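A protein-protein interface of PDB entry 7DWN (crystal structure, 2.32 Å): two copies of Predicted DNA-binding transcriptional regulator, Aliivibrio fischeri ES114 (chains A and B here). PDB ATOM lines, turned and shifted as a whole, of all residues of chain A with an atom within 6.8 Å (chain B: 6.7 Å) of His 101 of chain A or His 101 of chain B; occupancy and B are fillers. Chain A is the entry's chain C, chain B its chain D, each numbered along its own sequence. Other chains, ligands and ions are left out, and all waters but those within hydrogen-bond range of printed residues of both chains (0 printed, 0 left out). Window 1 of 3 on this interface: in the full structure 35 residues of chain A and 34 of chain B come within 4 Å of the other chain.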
ATOM      1  N   ALA A  99     -25.277  22.259   4.431  1.00  0.00           N
ATOM      2  CA  ALA A  99     -25.080  21.755   3.080  1.00  0.00           C
ATOM      3  C   ALA A  99     -24.888  20.247   3.081  1.00  0.00           C
ATOM      4  O   ALA A  99     -24.399  19.663   4.052  1.00  0.00           O
ATOM      5  CB  ALA A  99     -23.882  22.430   2.403  1.00  0.00           C
ATOM      6  N   ALA A 100     -25.283  19.625   1.972  1.00  0.00           N
ATOM      7  CA  ALA A 100     -24.945  18.233   1.732  1.00  0.00           C
ATOM      8  C   ALA A 100     -23.443  18.100   1.514  1.00  0.00           C
ATOM      9  O   ALA A 100     -22.812  18.971   0.907  1.00  0.00           O
ATOM     10  CB  ALA A 100     -25.712  17.696   0.524  1.00  0.00           C
ATOM     11  N   HIS A 101     -22.877  16.998   2.013  1.00  0.00           N
ATOM     12  CA  HIS A 101     -21.425  16.847   2.068  1.00  0.00           C
ATOM     13  C   HIS A 101     -20.782  17.043   0.699  1.00  0.00           C
ATOM     14  O   HIS A 101     -19.830  17.818   0.552  1.00  0.00           O
ATOM     15  CB  HIS A 101     -21.070  15.472   2.634  1.00  0.00           C
ATOM     16  CG  HIS A 101     -19.617  15.301   2.949  1.00  0.00           C
ATOM     17  ND1 HIS A 101     -19.138  15.245   4.240  1.00  0.00           N
ATOM     18  CD2 HIS A 101     -18.537  15.172   2.142  1.00  0.00           C
ATOM     19  CE1 HIS A 101     -17.826  15.088   4.215  1.00  0.00           C
ATOM     20  NE2 HIS A 101     -17.437  15.042   2.954  1.00  0.00           N
ATOM     21  N   SER A 102     -21.290  16.344  -0.317  1.00  0.00           N
ATOM     22  CA  SER A 102     -20.716  16.483  -1.651  1.00  0.00           C
ATOM     23  C   SER A 102     -20.964  17.877  -2.210  1.00  0.00           C
ATOM     24  O   SER A 102     -20.079  18.460  -2.848  1.00  0.00           O
ATOM     25  CB  SER A 102     -21.283  15.416  -2.588  1.00  0.00           C
ATOM     26  OG  SER A 102     -22.690  15.530  -2.713  1.00  0.00           O
ATOM     27  N   LEU A 103     -22.156  18.431  -1.968  1.00  0.00           N
ATOM     28  CA  LEU A 103     -22.433  19.802  -2.382  1.00  0.00           C
ATOM     29  C   LEU A 103     -21.458  20.769  -1.736  1.00  0.00           C
ATOM     30  O   LEU A 103     -20.939  21.678  -2.392  1.00  0.00           O
ATOM     31  CB  LEU A 103     -23.868  20.189  -2.027  1.00  0.00           C
ATOM     32  CG  LEU A 103     -24.945  19.487  -2.844  1.00  0.00           C
ATOM     33  CD1 LEU A 103     -26.281  20.165  -2.634  1.00  0.00           C
ATOM     34  CD2 LEU A 103     -24.559  19.476  -4.314  1.00  0.00           C
ATOM     35  N   ALA A 104     -21.195  20.586  -0.443  1.00  0.00           N
ATOM     36  CA  ALA A 104     -20.275  21.476   0.249  1.00  0.00           C
ATOM     37  C   ALA A 104     -18.868  21.358  -0.327  1.00  0.00           C
ATOM     38  O   ALA A 104     -18.261  22.361  -0.720  1.00  0.00           O
ATOM     39  CB  ALA A 104     -20.297  21.176   1.748  1.00  0.00           C
ATOM     40  N   THR A 105     -18.355  20.127  -0.434  1.00  0.00           N
ATOM     41  CA  THR A 105     -17.000  19.921  -0.940  1.00  0.00           C
ATOM     42  C   THR A 105     -16.847  20.379  -2.387  1.00  0.00           C
ATOM     43  O   THR A 105     -15.733  20.708  -2.811  1.00  0.00           O
ATOM     44  CB  THR A 105     -16.603  18.447  -0.817  1.00  0.00           C
ATOM     45  OG1 THR A 105     -17.548  17.627  -1.514  1.00  0.00           O
ATOM     46  CG2 THR A 105     -16.539  18.021   0.647  1.00  0.00           C
ATOM     47  N   SER A 106     -17.937  20.407  -3.158  1.00  0.00           N
ATOM     48  CA  SER A 106     -17.840  20.858  -4.540  1.00  0.00           C
ATOM     49  C   SER A 106     -17.949  22.375  -4.652  1.00  0.00           C
ATOM     50  O   SER A 106     -17.202  22.999  -5.415  1.00  0.00           O
ATOM     51  CB  SER A 106     -18.919  20.184  -5.390  1.00  0.00           C
ATOM     52  OG  SER A 106     -18.866  20.627  -6.735  1.00  0.00           O
ATOM     53  N   ALA A 128     -22.735  19.952   7.924  1.00  0.00           N
ATOM     54  CA  ALA A 128     -23.401  18.922   7.139  1.00  0.00           C
ATOM     55  C   ALA A 128     -24.908  18.976   7.358  1.00  0.00           C
ATOM     56  O   ALA A 128     -25.392  19.325   8.439  1.00  0.00           O
ATOM     57  CB  ALA A 128     -22.862  17.538   7.503  1.00  0.00           C
ATOM     58  N   ILE A 129     -25.654  18.628   6.311  1.00  0.00           N
ATOM     59  CA  ILE A 129     -27.099  18.804   6.330  1.00  0.00           C
ATOM     60  C   ILE A 129     -27.739  17.789   7.266  1.00  0.00           C
ATOM     61  O   ILE A 129     -27.340  16.617   7.319  1.00  0.00           O
ATOM     62  CB  ILE A 129     -27.668  18.690   4.904  1.00  0.00           C
ATOM     63  CG1 ILE A 129     -29.179  18.941   4.900  1.00  0.00           C
ATOM     64  CG2 ILE A 129     -27.348  17.328   4.296  1.00  0.00           C
ATOM     65  CD1 ILE A 129     -29.816  18.792   3.537  1.00  0.00           C
ATOM     66  N   LEU A 147     -27.571  24.459   1.194  1.00  0.00           N
ATOM     67  CA  LEU A 147     -27.187  23.885  -0.093  1.00  0.00           C
ATOM     68  C   LEU A 147     -27.691  22.447  -0.107  1.00  0.00           C
ATOM     69  O   LEU A 147     -27.117  21.574   0.547  1.00  0.00           O
ATOM     70  CB  LEU A 147     -25.678  23.949  -0.305  1.00  0.00           C
ATOM     71  CG  LEU A 147     -25.042  25.317  -0.527  1.00  0.00           C
ATOM     72  CD1 LEU A 147     -23.534  25.177  -0.617  1.00  0.00           C
ATOM     73  CD2 LEU A 147     -25.591  25.951  -1.786  1.00  0.00           C
ATOM     74  N   PHE A 149     -30.321  19.296  -2.403  1.00  0.00           N
ATOM     75  CA  PHE A 149     -30.774  18.849  -3.707  1.00  0.00           C
ATOM     76  C   PHE A 149     -32.252  19.192  -3.881  1.00  0.00           C
ATOM     77  O   PHE A 149     -32.892  19.766  -2.996  1.00  0.00           O
ATOM     78  CB  PHE A 149     -30.509  17.355  -3.883  1.00  0.00           C
ATOM     79  CG  PHE A 149     -29.049  17.005  -3.924  1.00  0.00           C
ATOM     80  CD1 PHE A 149     -28.341  17.061  -5.113  1.00  0.00           C
ATOM     81  CD2 PHE A 149     -28.380  16.632  -2.770  1.00  0.00           C
ATOM     82  CE1 PHE A 149     -26.998  16.748  -5.150  1.00  0.00           C
ATOM     83  CE2 PHE A 149     -27.039  16.318  -2.803  1.00  0.00           C
ATOM     84  CZ  PHE A 149     -26.347  16.377  -3.994  1.00  0.00           C
ATOM     85  N   MET A 223     -23.877   8.182   1.659  1.00  0.00           N
ATOM     86  CA  MET A 223     -22.727   9.031   1.378  1.00  0.00           C
ATOM     87  C   MET A 223     -22.176   8.702  -0.005  1.00  0.00           C
ATOM     88  O   MET A 223     -21.726   7.577  -0.248  1.00  0.00           O
ATOM     89  CB  MET A 223     -21.654   8.839   2.449  1.00  0.00           C
ATOM     90  CG  MET A 223     -22.123   9.181   3.859  1.00  0.00           C
ATOM     91  SD  MET A 223     -20.964   8.680   5.147  1.00  0.00           S
ATOM     92  CE  MET A 223     -21.267   6.916   5.217  1.00  0.00           C
ATOM     93  N   THR A 224     -22.204   9.687  -0.908  1.00  0.00           N
ATOM     94  CA  THR A 224     -21.693   9.459  -2.256  1.00  0.00           C
ATOM     95  C   THR A 224     -20.179   9.284  -2.258  1.00  0.00           C
ATOM     96  O   THR A 224     -19.635   8.608  -3.139  1.00  0.00           O
ATOM     97  CB  THR A 224     -22.103  10.606  -3.185  1.00  0.00           C
ATOM     98  OG1 THR A 224     -21.875  10.219  -4.544  1.00  0.00           O
ATOM     99  CG2 THR A 224     -21.298  11.861  -2.894  1.00  0.00           C
ATOM    100  N   ASP A 225     -19.487   9.875  -1.282  1.00  0.00           N
ATOM    101  CA  ASP A 225     -18.051   9.653  -1.154  1.00  0.00           C
ATOM    102  C   ASP A 225     -17.756   8.183  -0.885  1.00  0.00           C
ATOM    103  O   ASP A 225     -16.781   7.625  -1.405  1.00  0.00           O
ATOM    104  CB  ASP A 225     -17.498  10.537  -0.033  1.00  0.00           C
ATOM    105  CG  ASP A 225     -16.046  10.922  -0.245  1.00  0.00           C
ATOM    106  OD1 ASP A 225     -15.512  10.664  -1.345  1.00  0.00           O
ATOM    107  OD2 ASP A 225     -15.441  11.488   0.692  1.00  0.00           O
ATOM    108  N   MET A 226     -18.610   7.537  -0.089  1.00  0.00           N
ATOM    109  CA  MET A 226     -18.450   6.120   0.219  1.00  0.00           C
ATOM    110  C   MET A 226     -18.615   5.260  -1.028  1.00  0.00           C
ATOM    111  O   MET A 226     -17.793   4.372  -1.297  1.00  0.00           O
ATOM    112  CB  MET A 226     -19.467   5.720   1.289  1.00  0.00           C
ATOM    113  CG  MET A 226     -19.305   4.319   1.836  1.00  0.00           C
ATOM    114  SD  MET A 226     -17.852   4.165   2.884  1.00  0.00           S
ATOM    115  CE  MET A 226     -17.813   5.801   3.597  1.00  0.00           C
ATOM    116  N   TYR A 243     -20.236  15.778 -10.878  1.00  0.00           N
ATOM    117  CA  TYR A 243     -19.300  16.712 -10.263  1.00  0.00           C
ATOM    118  C   TYR A 243     -18.366  16.047  -9.259  1.00  0.00           C
ATOM    119  O   TYR A 243     -17.394  16.682  -8.835  1.00  0.00           O
ATOM    120  CB  TYR A 243     -20.062  17.857  -9.583  1.00  0.00           C
ATOM    121  CG  TYR A 243     -20.974  17.436  -8.445  1.00  0.00           C
ATOM    122  CD1 TYR A 243     -20.469  17.218  -7.166  1.00  0.00           C
ATOM    123  CD2 TYR A 243     -22.342  17.281  -8.645  1.00  0.00           C
ATOM    124  CE1 TYR A 243     -21.295  16.840  -6.125  1.00  0.00           C
ATOM    125  CE2 TYR A 243     -23.178  16.909  -7.607  1.00  0.00           C
ATOM    126  CZ  TYR A 243     -22.648  16.688  -6.351  1.00  0.00           C
ATOM    127  OH  TYR A 243     -23.472  16.316  -5.315  1.00  0.00           O
ATOM    128  N   ALA B  99     -21.950   6.110  11.143  1.00  0.00           N
ATOM    129  CA  ALA B  99     -20.530   6.418  11.230  1.00  0.00           C
ATOM    130  C   ALA B  99     -20.266   7.874  10.887  1.00  0.00           C
ATOM    131  O   ALA B  99     -20.930   8.449  10.021  1.00  0.00           O
ATOM    132  CB  ALA B  99     -19.711   5.512  10.302  1.00  0.00           C
ATOM    133  N   ALA B 100     -19.289   8.460  11.577  1.00  0.00           N
ATOM    134  CA  ALA B 100     -18.746   9.741  11.154  1.00  0.00           C
ATOM    135  C   ALA B 100     -18.094   9.587   9.788  1.00  0.00           C
ATOM    136  O   ALA B 100     -17.438   8.579   9.506  1.00  0.00           O
ATOM    137  CB  ALA B 100     -17.736  10.259  12.178  1.00  0.00           C
ATOM    138  N   HIS B 101     -18.279  10.604   8.942  1.00  0.00           N
ATOM    139  CA  HIS B 101     -17.928  10.516   7.525  1.00  0.00           C
ATOM    140  C   HIS B 101     -16.494  10.031   7.318  1.00  0.00           C
ATOM    141  O   HIS B 101     -16.247   9.086   6.557  1.00  0.00           O
ATOM    142  CB  HIS B 101     -18.138  11.888   6.881  1.00  0.00           C
ATOM    143  CG  HIS B 101     -18.236  11.855   5.390  1.00  0.00           C
ATOM    144  ND1 HIS B 101     -17.132  11.735   4.575  1.00  0.00           N
ATOM    145  CD2 HIS B 101     -19.305  11.949   4.565  1.00  0.00           C
ATOM    146  CE1 HIS B 101     -17.517  11.745   3.312  1.00  0.00           C
ATOM    147  NE2 HIS B 101     -18.832  11.873   3.279  1.00  0.00           N
ATOM    148  N   SER B 102     -15.534  10.663   8.001  1.00  0.00           N
ATOM    149  CA  SER B 102     -14.132  10.304   7.809  1.00  0.00           C
ATOM    150  C   SER B 102     -13.842   8.892   8.303  1.00  0.00           C
ATOM    151  O   SER B 102     -13.091   8.148   7.661  1.00  0.00           O
ATOM    152  CB  SER B 102     -13.223  11.314   8.512  1.00  0.00           C
ATOM    153  OG  SER B 102     -13.437  11.325   9.912  1.00  0.00           O
ATOM    154  N   LEU B 103     -14.427   8.504   9.439  1.00  0.00           N
ATOM    155  CA  LEU B 103     -14.242   7.143   9.934  1.00  0.00           C
ATOM    156  C   LEU B 103     -14.816   6.126   8.962  1.00  0.00           C
ATOM    157  O   LEU B 103     -14.223   5.066   8.736  1.00  0.00           O
ATOM    158  CB  LEU B 103     -14.892   6.982  11.305  1.00  0.00           C
ATOM    159  CG  LEU B 103     -14.266   7.778  12.445  1.00  0.00           C
ATOM    160  CD1 LEU B 103     -14.916   7.401  13.764  1.00  0.00           C
ATOM    161  CD2 LEU B 103     -12.763   7.549  12.492  1.00  0.00           C
ATOM    162  N   ALA B 104     -15.980   6.427   8.387  1.00  0.00           N
ATOM    163  CA  ALA B 104     -16.562   5.525   7.404  1.00  0.00           C
ATOM    164  C   ALA B 104     -15.637   5.370   6.201  1.00  0.00           C
ATOM    165  O   ALA B 104     -15.248   4.251   5.848  1.00  0.00           O
ATOM    166  CB  ALA B 104     -17.943   6.029   6.989  1.00  0.00           C
ATOM    167  N   THR B 105     -15.232   6.493   5.594  1.00  0.00           N
ATOM    168  CA  THR B 105     -14.337   6.443   4.438  1.00  0.00           C
ATOM    169  C   THR B 105     -12.990   5.801   4.756  1.00  0.00           C
ATOM    170  O   THR B 105     -12.333   5.290   3.842  1.00  0.00           O
ATOM    171  CB  THR B 105     -14.104   7.850   3.877  1.00  0.00           C
ATOM    172  OG1 THR B 105     -13.612   8.708   4.915  1.00  0.00           O
ATOM    173  CG2 THR B 105     -15.391   8.428   3.309  1.00  0.00           C
ATOM    174  N   SER B 106     -12.559   5.819   6.018  1.00  0.00           N
ATOM    175  CA  SER B 106     -11.272   5.236   6.378  1.00  0.00           C
ATOM    176  C   SER B 106     -11.361   3.745   6.686  1.00  0.00           C
ATOM    177  O   SER B 106     -10.439   2.992   6.357  1.00  0.00           O
ATOM    178  CB  SER B 106     -10.677   5.979   7.579  1.00  0.00           C
ATOM    179  OG  SER B 106      -9.420   5.434   7.947  1.00  0.00           O
ATOM    180  N   ALA B 128     -24.523   8.352   7.639  1.00  0.00           N
ATOM    181  CA  ALA B 128     -23.795   9.392   8.353  1.00  0.00           C
ATOM    182  C   ALA B 128     -24.411   9.621   9.726  1.00  0.00           C
ATOM    183  O   ALA B 128     -25.635   9.636   9.883  1.00  0.00           O
ATOM    184  CB  ALA B 128     -23.793  10.690   7.549  1.00  0.00           C
ATOM    185  N   ILE B 129     -23.556   9.805  10.721  1.00  0.00           N
ATOM    186  CA  ILE B 129     -23.977   9.822  12.116  1.00  0.00           C
ATOM    187  C   ILE B 129     -24.415  11.223  12.519  1.00  0.00           C
ATOM    188  O   ILE B 129     -23.866  12.230  12.052  1.00  0.00           O
ATOM    189  CB  ILE B 129     -22.850   9.304  13.033  1.00  0.00           C
ATOM    190  CG1 ILE B 129     -23.388   9.078  14.443  1.00  0.00           C
ATOM    191  CG2 ILE B 129     -21.691  10.280  13.084  1.00  0.00           C
ATOM    192  CD1 ILE B 129     -24.706   8.357  14.449  1.00  0.00           C
ATOM    193  N   LEU B 147     -19.835   3.844  14.614  1.00  0.00           N
ATOM    194  CA  LEU B 147     -18.425   4.199  14.465  1.00  0.00           C
ATOM    195  C   LEU B 147     -18.297   5.682  14.784  1.00  0.00           C
ATOM    196  O   LEU B 147     -18.671   6.534  13.974  1.00  0.00           O
ATOM    197  CB  LEU B 147     -17.919   3.884  13.061  1.00  0.00           C
ATOM    198  CG  LEU B 147     -17.650   2.416  12.746  1.00  0.00           C
ATOM    199  CD1 LEU B 147     -17.114   2.274  11.334  1.00  0.00           C
ATOM    200  CD2 LEU B 147     -16.674   1.833  13.754  1.00  0.00           C
ATOM    201  N   PHE B 149     -16.255   8.859  17.631  1.00  0.00           N
ATOM    202  CA  PHE B 149     -15.068   9.183  18.400  1.00  0.00           C
ATOM    203  C   PHE B 149     -15.359   9.056  19.894  1.00  0.00           C
ATOM    204  O   PHE B 149     -16.471   8.718  20.310  1.00  0.00           O
ATOM    205  CB  PHE B 149     -14.562  10.574  18.030  1.00  0.00           C
ATOM    206  CG  PHE B 149     -14.101  10.680  16.607  1.00  0.00           C
ATOM    207  CD1 PHE B 149     -12.840  10.239  16.239  1.00  0.00           C
ATOM    208  CD2 PHE B 149     -14.934  11.204  15.634  1.00  0.00           C
ATOM    209  CE1 PHE B 149     -12.416  10.327  14.927  1.00  0.00           C
ATOM    210  CE2 PHE B 149     -14.517  11.296  14.321  1.00  0.00           C
ATOM    211  CZ  PHE B 149     -13.257  10.855  13.967  1.00  0.00           C
ATOM    212  N   MET B 223     -16.921  19.151   9.056  1.00  0.00           N
ATOM    213  CA  MET B 223     -16.488  18.094   8.148  1.00  0.00           C
ATOM    214  C   MET B 223     -14.988  18.216   7.915  1.00  0.00           C
ATOM    215  O   MET B 223     -14.524  19.209   7.344  1.00  0.00           O
ATOM    216  CB  MET B 223     -17.250  18.177   6.826  1.00  0.00           C
ATOM    217  CG  MET B 223     -18.759  18.066   6.989  1.00  0.00           C
ATOM    218  SD  MET B 223     -19.689  18.424   5.486  1.00  0.00           S
ATOM    219  CE  MET B 223     -19.541  20.206   5.400  1.00  0.00           C
ATOM    220  N   THR B 224     -14.235  17.202   8.355  1.00  0.00           N
ATOM    221  CA  THR B 224     -12.796  17.187   8.115  1.00  0.00           C
ATOM    222  C   THR B 224     -12.472  17.257   6.629  1.00  0.00           C
ATOM    223  O   THR B 224     -11.468  17.861   6.243  1.00  0.00           O
ATOM    224  CB  THR B 224     -12.168  15.935   8.737  1.00  0.00           C
ATOM    225  OG1 THR B 224     -12.083  16.088  10.159  1.00  0.00           O
ATOM    226  CG2 THR B 224     -10.783  15.670   8.170  1.00  0.00           C
ATOM    227  N   ASP B 225     -13.311  16.658   5.780  1.00  0.00           N
ATOM    228  CA  ASP B 225     -13.057  16.697   4.343  1.00  0.00           C
ATOM    229  C   ASP B 225     -13.049  18.130   3.827  1.00  0.00           C
ATOM    230  O   ASP B 225     -12.243  18.482   2.957  1.00  0.00           O
ATOM    231  CB  ASP B 225     -14.104  15.863   3.606  1.00  0.00           C
ATOM    232  CG  ASP B 225     -13.581  15.287   2.303  1.00  0.00           C
ATOM    233  OD1 ASP B 225     -12.354  15.354   2.069  1.00  0.00           O
ATOM    234  OD2 ASP B 225     -14.398  14.766   1.512  1.00  0.00           O
ATOM    235  N   MET B 226     -13.930  18.975   4.364  1.00  0.00           N
ATOM    236  CA  MET B 226     -13.969  20.376   3.958  1.00  0.00           C
ATOM    237  C   MET B 226     -12.684  21.099   4.342  1.00  0.00           C
ATOM    238  O   MET B 226     -12.082  21.806   3.521  1.00  0.00           O
ATOM    239  CB  MET B 226     -15.178  21.061   4.594  1.00  0.00           C
ATOM    240  CG  MET B 226     -15.371  22.499   4.158  1.00  0.00           C
ATOM    241  SD  MET B 226     -15.826  22.589   2.423  1.00  0.00           S
ATOM    242  CE  MET B 226     -16.950  21.206   2.370  1.00  0.00           C
ATOM    243  N   TYR B 243      -5.189   9.745   9.747  1.00  0.00           N
ATOM    244  CA  TYR B 243      -5.712   8.757   8.810  1.00  0.00           C
ATOM    245  C   TYR B 243      -6.325   9.380   7.563  1.00  0.00           C
ATOM    246  O   TYR B 243      -6.581   8.653   6.597  1.00  0.00           O
ATOM    247  CB  TYR B 243      -6.746   7.862   9.503  1.00  0.00           C
ATOM    248  CG  TYR B 243      -7.983   8.573  10.018  1.00  0.00           C
ATOM    249  CD1 TYR B 243      -9.027   8.909   9.163  1.00  0.00           C
ATOM    250  CD2 TYR B 243      -8.121   8.879  11.365  1.00  0.00           C
ATOM    251  CE1 TYR B 243     -10.159   9.550   9.630  1.00  0.00           C
ATOM    252  CE2 TYR B 243      -9.256   9.515  11.842  1.00  0.00           C
ATOM    253  CZ  TYR B 243     -10.268   9.850  10.967  1.00  0.00           C
ATOM    254  OH  TYR B 243     -11.398  10.485  11.430  1.00  0.00           O
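OG1 of Thr 105 of chain B lies within hydrogen-bond range of O of Ser 102 of chain B, at 2.9 Å. O of His 101 of chain B sits at hydrogen-bond distance from OG1 of Thr 105 of chain B, at 3.1 Å. OG1 of Thr 105 of chain A sits at hydrogen-bond distance from O of His 101 of chain A. O of Ser 102 of chain A sits at hydrogen-bond distance from OG1 of Thr 105 of chain A (3.0 Å).
Among the printed residues, merely in contact across the chains: Ala 104 of chain A with Met 226 of chain B, Thr 105 of chain A with Met 226 of chain B, Met 226 of chain A with Thr 105 of chain B, Asp 225 of chain A with His 101 of chain B, Met 226 of chain A with Ala 104 of chain B, Asp 225 of chain A with Asp 225 of chain B, Met 223 of chain A with His 101 of chain B, Ala 104 of chain A with Met 223 of chain B, Ala 128 of chain A with Met 223 of chain B, Met 223 of chain A with Ala 104 of chain B and Thr 105 of chain A with Asp 225 of chain B.
His 101 of chain B touches its own counterpart, His 101 of chain A. His 101 of chain A touches Asp 225 of chain B, and with the chains exchanged Asp 225 of chain A touches His 101 of chain B. Ala 104 of chain A touches Met 226 of chain B, and with the chains exchanged Met 226 of chain A touches Ala 104 of chain B. Asp 225 of chain B touches its own counterpart, Asp 225 of chain A.
A ring nitrogen (ND1) of His 101 of chain A lies within hydrogen-bond range of the side-chain sulfur of Met 223 of chain B. The side-chain carboxylate (OD2) of Asp 225 of chain B is in hydrogen-bond range of a ring nitrogen (NE2) of His 101 of chain A, at 3.4 Å. A ring nitrogen (NE2) of His 101 of chain A sits close to a ring nitrogen (NE2) of His 101 of chain B, at 3.5 Å.
Of chain B, only His 101 (3.3 Å), Met 223 (3.5 Å) and Asp 225 (3.4 Å) come within 4 Å of His 101 of chain A. His 101 of chain B touches just these residues of chain A: His 101, Met 223 and Asp 225. Printed residues of chain B within 4 Å of Asp 225 of chain A: His 101 and Asp 225. Of the printed residues of chain A, Thr 105 of chain B touches Met 226 (3.3 Å). Printed residues of chain A within 4 Å of Asp 225 of chain B: His 101, Thr 105 and Asp 225. Leu 103 of chain B touches none of the printed residues of chain A. The nearest printed residue of chain A that does not touch Asp 225 of chain B is Ser 102 of chain A (7.3 Å).
Of the 17 printed residues of chain A, 7 touch a printed residue of chain B. Printed residues of chain A that touch a printed residue of chain B: His 101, Ala 104, Thr 105, Ala 128, Met 223, Asp 225 and Met 226. Hydrophobic or aromatic side chains of chain A that line the printed part of chain B: His 101, Ala 104, Ala 128, Met 223 and Met 226. Hydrophobic or aromatic side chains of chain B within 4 Å of the printed part of chain A: His 101, Ala 104, Met 223 and Met 226.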
